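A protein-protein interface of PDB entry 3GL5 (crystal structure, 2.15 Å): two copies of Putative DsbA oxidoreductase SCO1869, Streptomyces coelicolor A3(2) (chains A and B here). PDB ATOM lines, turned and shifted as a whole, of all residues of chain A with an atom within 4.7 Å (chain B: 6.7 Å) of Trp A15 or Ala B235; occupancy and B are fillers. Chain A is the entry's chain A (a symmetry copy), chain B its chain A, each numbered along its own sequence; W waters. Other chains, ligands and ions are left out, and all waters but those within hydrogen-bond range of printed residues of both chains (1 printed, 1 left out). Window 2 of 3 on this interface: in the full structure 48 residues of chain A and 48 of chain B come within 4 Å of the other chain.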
ATOM      1  N   CYS A  13       7.400   3.299 -11.702  1.00  0.00           N
ATOM      2  CA  CYS A  13       7.962   1.987 -11.410  1.00  0.00           C
ATOM      3  C   CYS A  13       9.496   2.152 -11.391  1.00  0.00           C
ATOM      4  O   CYS A  13      10.114   2.260 -12.439  1.00  0.00           O
ATOM      5  CB  CYS A  13       7.492   1.038 -12.498  1.00  0.00           C
ATOM      6  SG  CYS A  13       8.314  -0.500 -12.674  1.00  0.00           S
ATOM      7  N   PRO A  14      10.095   2.236 -10.201  1.00  0.00           N
ATOM      8  CA  PRO A  14      11.553   2.477 -10.110  1.00  0.00           C
ATOM      9  C   PRO A  14      12.377   1.422 -10.837  1.00  0.00           C
ATOM     10  O   PRO A  14      13.356   1.779 -11.452  1.00  0.00           O
ATOM     11  CB  PRO A  14      11.843   2.433  -8.598  1.00  0.00           C
ATOM     12  CG  PRO A  14      10.527   2.624  -7.907  1.00  0.00           C
ATOM     13  CD  PRO A  14       9.418   2.241  -8.881  1.00  0.00           C
ATOM     14  N   TRP A  15      11.994   0.141 -10.763  1.00  0.00           N
ATOM     15  CA  TRP A  15      12.669  -0.951 -11.489  1.00  0.00           C
ATOM     16  C   TRP A  15      12.504  -0.937 -12.995  1.00  0.00           C
ATOM     17  O   TRP A  15      13.282  -1.575 -13.683  1.00  0.00           O
ATOM     18  CB  TRP A  15      12.199  -2.317 -10.974  1.00  0.00           C
ATOM     19  CG  TRP A  15      12.654  -2.537  -9.525  1.00  0.00           C
ATOM     20  CD1 TRP A  15      11.871  -2.608  -8.390  1.00  0.00           C
ATOM     21  CD2 TRP A  15      14.003  -2.630  -9.089  1.00  0.00           C
ATOM     22  NE1 TRP A  15      12.677  -2.762  -7.266  1.00  0.00           N
ATOM     23  CE2 TRP A  15      13.987  -2.779  -7.678  1.00  0.00           C
ATOM     24  CE3 TRP A  15      15.229  -2.624  -9.763  1.00  0.00           C
ATOM     25  CZ2 TRP A  15      15.161  -2.934  -6.927  1.00  0.00           C
ATOM     26  CZ3 TRP A  15      16.411  -2.759  -9.007  1.00  0.00           C
ATOM     27  CH2 TRP A  15      16.357  -2.915  -7.604  1.00  0.00           C
ATOM     28  N   CYS A  16      11.447  -0.291 -13.497  1.00  0.00           N
ATOM     29  CA  CYS A  16      11.277  -0.075 -14.938  1.00  0.00           C
ATOM     30  C   CYS A  16      12.367   0.892 -15.423  1.00  0.00           C
ATOM     31  O   CYS A  16      13.033   0.634 -16.433  1.00  0.00           O
ATOM     32  CB  CYS A  16       9.883   0.490 -15.221  1.00  0.00           C
ATOM     33  SG  CYS A  16       8.555  -0.637 -14.825  1.00  0.00           S
ATOM     34  N   TYR A  17      12.550   1.985 -14.675  1.00  0.00           N
ATOM     35  CA  TYR A  17      13.589   2.996 -14.917  1.00  0.00           C
ATOM     36  C   TYR A  17      15.010   2.434 -14.841  1.00  0.00           C
ATOM     37  O   TYR A  17      15.809   2.671 -15.744  1.00  0.00           O
ATOM     38  CB  TYR A  17      13.420   4.108 -13.904  1.00  0.00           C
ATOM     39  CG  TYR A  17      14.378   5.306 -13.969  1.00  0.00           C
ATOM     40  CD1 TYR A  17      14.645   6.013 -15.168  1.00  0.00           C
ATOM     41  CD2 TYR A  17      14.933   5.780 -12.809  1.00  0.00           C
ATOM     42  CE1 TYR A  17      15.524   7.168 -15.162  1.00  0.00           C
ATOM     43  CE2 TYR A  17      15.757   6.904 -12.780  1.00  0.00           C
ATOM     44  CZ  TYR A  17      16.055   7.588 -13.931  1.00  0.00           C
ATOM     45  OH  TYR A  17      16.858   8.686 -13.764  1.00  0.00           O
ATOM     46  N   VAL A  18      15.315   1.684 -13.775  1.00  0.00           N
ATOM     47  CA  VAL A  18      16.612   1.010 -13.640  1.00  0.00           C
ATOM     48  C   VAL A  18      16.766  -0.115 -14.687  1.00  0.00           C
ATOM     49  O   VAL A  18      17.818  -0.207 -15.345  1.00  0.00           O
ATOM     50  CB  VAL A  18      16.896   0.495 -12.163  1.00  0.00           C
ATOM     51  CG1 VAL A  18      18.281  -0.081 -12.030  1.00  0.00           C
ATOM     52  CG2 VAL A  18      16.785   1.654 -11.171  1.00  0.00           C
ATOM     53  N   GLY A  19      15.727  -0.942 -14.858  1.00  0.00           N
ATOM     54  CA  GLY A  19      15.780  -2.045 -15.834  1.00  0.00           C
ATOM     55  C   GLY A  19      15.914  -1.638 -17.298  1.00  0.00           C
ATOM     56  O   GLY A  19      16.462  -2.393 -18.148  1.00  0.00           O
ATOM     57  N   LYS A  20      15.408  -0.463 -17.637  1.00  0.00           N
ATOM     58  CA  LYS A  20      15.566   0.004 -18.998  1.00  0.00           C
ATOM     59  C   LYS A  20      17.070   0.218 -19.296  1.00  0.00           C
ATOM     60  O   LYS A  20      17.583  -0.205 -20.330  1.00  0.00           O
ATOM     61  CB  LYS A  20      14.794   1.307 -19.242  1.00  0.00           C
ATOM     62  CG  LYS A  20      15.053   1.844 -20.695  1.00  0.00           C
ATOM     63  CD  LYS A  20      13.960   2.773 -21.137  1.00  0.00           C
ATOM     64  CE  LYS A  20      14.417   4.159 -21.090  1.00  0.00           C
ATOM     65  NZ  LYS A  20      15.301   4.385 -22.280  1.00  0.00           N
ATOM     66  N   ARG A  22      19.624  -1.080 -17.689  1.00  0.00           N
ATOM     67  CA  ARG A  22      20.320  -2.372 -17.641  1.00  0.00           C
ATOM     68  C   ARG A  22      20.192  -3.131 -18.970  1.00  0.00           C
ATOM     69  O   ARG A  22      21.165  -3.693 -19.470  1.00  0.00           O
ATOM     70  CB  ARG A  22      19.847  -3.219 -16.453  1.00  0.00           C
ATOM     71  CG  ARG A  22      20.680  -3.016 -15.272  1.00  0.00           C
ATOM     72  CD  ARG A  22      20.170  -3.724 -14.047  1.00  0.00           C
ATOM     73  NE  ARG A  22      20.681  -3.102 -12.827  1.00  0.00           N
ATOM     74  CZ  ARG A  22      20.291  -3.454 -11.602  1.00  0.00           C
ATOM     75  NH1 ARG A  22      19.377  -4.388 -11.433  1.00  0.00           N
ATOM     76  NH2 ARG A  22      20.783  -2.852 -10.537  1.00  0.00           N
ATOM     77  N   ASN A  78      18.676   1.988  -1.499  1.00  0.00           N
ATOM     78  CA  ASN A  78      19.182   0.969  -2.378  1.00  0.00           C
ATOM     79  C   ASN A  78      18.893   1.246  -3.847  1.00  0.00           C
ATOM     80  O   ASN A  78      19.760   1.057  -4.707  1.00  0.00           O
ATOM     81  CB  ASN A  78      18.621  -0.398  -2.046  1.00  0.00           C
ATOM     82  CG  ASN A  78      19.049  -1.423  -3.076  1.00  0.00           C
ATOM     83  OD1 ASN A  78      20.243  -1.565  -3.359  1.00  0.00           O
ATOM     84  ND2 ASN A  78      18.078  -2.130  -3.663  1.00  0.00           N
ATOM     85  N   LEU A  79      17.673   1.689  -4.132  1.00  0.00           N
ATOM     86  CA  LEU A  79      17.300   2.024  -5.491  1.00  0.00           C
ATOM     87  C   LEU A  79      18.159   3.183  -6.008  1.00  0.00           C
ATOM     88  O   LEU A  79      18.552   3.203  -7.165  1.00  0.00           O
ATOM     89  CB  LEU A  79      15.805   2.331  -5.563  1.00  0.00           C
ATOM     90  CG  LEU A  79      14.937   1.091  -5.859  1.00  0.00           C
ATOM     91  CD1 LEU A  79      13.457   1.334  -5.447  1.00  0.00           C
ATOM     92  CD2 LEU A  79      15.038   0.763  -7.329  1.00  0.00           C
ATOM     93  N   GLN A  82      21.548   1.744  -7.033  1.00  0.00           N
ATOM     94  CA  GLN A  82      21.541   0.931  -8.240  1.00  0.00           C
ATOM     95  C   GLN A  82      21.282   1.804  -9.476  1.00  0.00           C
ATOM     96  O   GLN A  82      21.829   1.540 -10.555  1.00  0.00           O
ATOM     97  CB  GLN A  82      20.527  -0.216  -8.128  1.00  0.00           C
ATOM     98  CG  GLN A  82      20.776  -1.172  -6.942  1.00  0.00           C
ATOM     99  CD  GLN A  82      20.061  -2.502  -7.098  1.00  0.00           C
ATOM    100  OE1 GLN A  82      19.984  -3.053  -8.188  1.00  0.00           O
ATOM    101  NE2 GLN A  82      19.544  -3.026  -6.004  1.00  0.00           N
ATOM    102  N   PRO A 185       9.331  -4.220 -14.852  1.00  0.00           N
ATOM    103  CA  PRO A 185       9.400  -4.285 -16.321  1.00  0.00           C
ATOM    104  C   PRO A 185       9.272  -5.731 -16.813  1.00  0.00           C
ATOM    105  O   PRO A 185       9.597  -6.681 -16.072  1.00  0.00           O
ATOM    106  CB  PRO A 185      10.794  -3.697 -16.622  1.00  0.00           C
ATOM    107  CG  PRO A 185      11.608  -4.149 -15.418  1.00  0.00           C
ATOM    108  CD  PRO A 185      10.679  -4.058 -14.256  1.00  0.00           C
ATOM    109  N   ALA A 198      14.067  -6.062 -13.217  1.00  0.00           N
ATOM    110  CA  ALA A 198      15.352  -5.412 -13.521  1.00  0.00           C
ATOM    111  C   ALA A 198      16.540  -6.363 -13.284  1.00  0.00           C
ATOM    112  O   ALA A 198      17.324  -6.233 -12.343  1.00  0.00           O
ATOM    113  CB  ALA A 198      15.519  -4.119 -12.724  1.00  0.00           C
ATOM    114  N   ALA B 226      15.616  -9.436 -11.656  1.00  0.00           N
ATOM    115  CA  ALA B 226      14.590 -10.149 -10.882  1.00  0.00           C
ATOM    116  C   ALA B 226      13.598  -9.178 -10.251  1.00  0.00           C
ATOM    117  O   ALA B 226      12.380  -9.407 -10.308  1.00  0.00           O
ATOM    118  CB  ALA B 226      15.223 -11.089  -9.817  1.00  0.00           C
ATOM    119  N   GLU B 227      14.124  -8.086  -9.687  1.00  0.00           N
ATOM    120  CA  GLU B 227      13.318  -7.040  -9.046  1.00  0.00           C
ATOM    121  C   GLU B 227      12.287  -6.403  -9.982  1.00  0.00           C
ATOM    122  O   GLU B 227      12.623  -5.959 -11.073  1.00  0.00           O
ATOM    123  CB  GLU B 227      14.222  -5.959  -8.465  1.00  0.00           C
ATOM    124  CG  GLU B 227      14.884  -6.346  -7.156  1.00  0.00           C
ATOM    125  CD  GLU B 227      16.284  -6.917  -7.324  1.00  0.00           C
ATOM    126  OE1 GLU B 227      16.608  -7.514  -8.388  1.00  0.00           O
ATOM    127  OE2 GLU B 227      17.075  -6.759  -6.366  1.00  0.00           O
ATOM    128  N   ALA B 228      11.039  -6.366  -9.528  1.00  0.00           N
ATOM    129  CA  ALA B 228       9.906  -5.932 -10.343  1.00  0.00           C
ATOM    130  C   ALA B 228       8.914  -5.152  -9.485  1.00  0.00           C
ATOM    131  O   ALA B 228       9.006  -5.172  -8.261  1.00  0.00           O
ATOM    132  CB  ALA B 228       9.221  -7.150 -10.968  1.00  0.00           C
ATOM    133  N   CYS B 229       7.983  -4.458 -10.138  1.00  0.00           N
ATOM    134  CA  CYS B 229       6.806  -3.889  -9.484  1.00  0.00           C
ATOM    135  C   CYS B 229       5.543  -4.639  -9.910  1.00  0.00           C
ATOM    136  O   CYS B 229       5.318  -4.890 -11.086  1.00  0.00           O
ATOM    137  CB  CYS B 229       6.698  -2.392  -9.759  1.00  0.00           C
ATOM    138  SG  CYS B 229       8.179  -1.445  -9.210  1.00  0.00           S
ATOM    139  N   GLY B 230       4.735  -5.012  -8.925  1.00  0.00           N
ATOM    140  CA  GLY B 230       3.637  -5.940  -9.147  1.00  0.00           C
ATOM    141  C   GLY B 230       2.428  -5.561  -8.329  1.00  0.00           C
ATOM    142  O   GLY B 230       2.421  -4.494  -7.728  1.00  0.00           O
ATOM    143  N   GLY B 233       3.207  -4.064  -4.952  1.00  0.00           N
ATOM    144  CA  GLY B 233       4.360  -3.141  -4.916  1.00  0.00           C
ATOM    145  C   GLY B 233       5.667  -3.642  -5.510  1.00  0.00           C
ATOM    146  O   GLY B 233       5.683  -4.629  -6.260  1.00  0.00           O
ATOM    147  N   CYS B 234       6.764  -2.961  -5.156  1.00  0.00           N
ATOM    148  CA  CYS B 234       8.109  -3.201  -5.740  1.00  0.00           C
ATOM    149  C   CYS B 234       9.070  -3.927  -4.804  1.00  0.00           C
ATOM    150  O   CYS B 234       8.952  -3.816  -3.584  1.00  0.00           O
ATOM    151  CB  CYS B 234       8.768  -1.878  -6.182  1.00  0.00           C
ATOM    152  SG  CYS B 234       7.746  -0.828  -7.280  1.00  0.00           S
ATOM    153  N   ALA B 235      10.037  -4.637  -5.389  1.00  0.00           N
ATOM    154  CA  ALA B 235      11.032  -5.420  -4.634  1.00  0.00           C
ATOM    155  C   ALA B 235      12.048  -4.546  -3.869  1.00  0.00           C
ATOM    156  O   ALA B 235      12.249  -3.374  -4.215  1.00  0.00           O
ATOM    157  CB  ALA B 235      11.759  -6.429  -5.567  1.00  0.00           C
ATOM    158  N   VAL B 236      12.665  -5.138  -2.833  1.00  0.00           N
ATOM    159  CA  VAL B 236      13.659  -4.482  -1.949  1.00  0.00           C
ATOM    160  C   VAL B 236      14.852  -5.395  -1.498  1.00  0.00           C
ATOM    161  O   VAL B 236      15.448  -5.143  -0.432  1.00  0.00           O
ATOM    162  CB  VAL B 236      12.986  -3.903  -0.643  1.00  0.00           C
ATOM    163  CG1 VAL B 236      12.183  -2.641  -0.926  1.00  0.00           C
ATOM    164  CG2 VAL B 236      12.129  -4.967   0.062  1.00  0.00           C
ATOM    165  N   PRO B 237      15.224  -6.427  -2.309  1.00  0.00           N
ATOM    166  CA  PRO B 237      16.073  -7.531  -1.784  1.00  0.00           C
ATOM    167  C   PRO B 237      17.481  -7.135  -1.276  1.00  0.00           C
ATOM    168  O   PRO B 237      17.757  -7.268  -0.073  1.00  0.00           O
ATOM    169  CB  PRO B 237      16.157  -8.521  -2.971  1.00  0.00           C
ATOM    170  CG  PRO B 237      15.062  -8.088  -3.934  1.00  0.00           C
ATOM    171  CD  PRO B 237      14.974  -6.594  -3.755  1.00  0.00           C
HETATM  172  O   HOH W   1      18.449  -7.735 -10.396  1.00  0.00           O
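No position is printed for both chains. Of the 10 pairs that touch across the chains among the printed residues, none has its exchanged pair printed and touching as well.
Water W1 bridges O of Ala A198 (2.7 Å) and OE1 of Glu B227 (2.7 Å).
Trp A15 touches just these residues of chain B: Glu B227, Ala B228, Cys B229, Cys B234 and Ala B235. Printed residues of chain B within 4 Å of Cys A13: Cys B229 (3.6 Å). Printed residues of chain A within 4 Å of Ala B226: Ala A198 (3.6 Å). The nearest residue of chain B that does not touch Trp A15 is Pro B237 (4.8 Å). The nearest printed residue of chain A that does not touch Ala B235 is Leu A79 (5.0 Å).
Hydrophobic or aromatic side chains of chain A that line the printed part of chain B: Pro A14, Trp A15 and Ala A198. Along chain A the printed residues that touch a printed residue of chain B span positions 13 to 198. Of the 10 printed residues of chain B, 6 touch a printed residue of chain A. Among the printed residues, no Asp or Glu carboxylate lies within 4 Å of a Lys or Arg side-chain nitrogen of the other chain.
The backbone NH (N) of Ala A198 sits at hydrogen-bond distance from the backbone carbonyl oxygen (O) of Glu B227, at 2.6 Å. O of Ala B235 is in hydrogen-bond range of NE1 of Trp A15, 3.1 Å away. SG of Cys A13 sits close to SG of Cys B229, at 3.6 Å.
The backbone carbonyl oxygen of Ala B228 lies within hydrogen-bond range of the backbone NH of Ala B235. The side-chain sulfur (SG) of Cys B229 is disulfide-bonded to the side-chain sulfur (SG) of Cys B234, at 2.1 Å. SG of Cys A13 is disulfide-bonded to SG of Cys A16, at 2.2 Å. The guanidinium group (NH1) of Arg A22 is in hydrogen-bond range of the backbone carbonyl oxygen (O) of Ala A198 (2.9 Å).
Among the printed residues, pairs that only touch across the chains: Trp A15 with Glu B227 (3.3 Å), Ala A198 with Ala B226 (3.6 Å), Pro A14 with Cys B234 (3.8 Å), Trp A15 with Ala B228 (3.8 Å), Trp A15 with Cys B234 (3.9 Å), Pro A14 with Cys B229 (3.9 Å) and Trp A15 with Cys B229 (3.96 Å).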
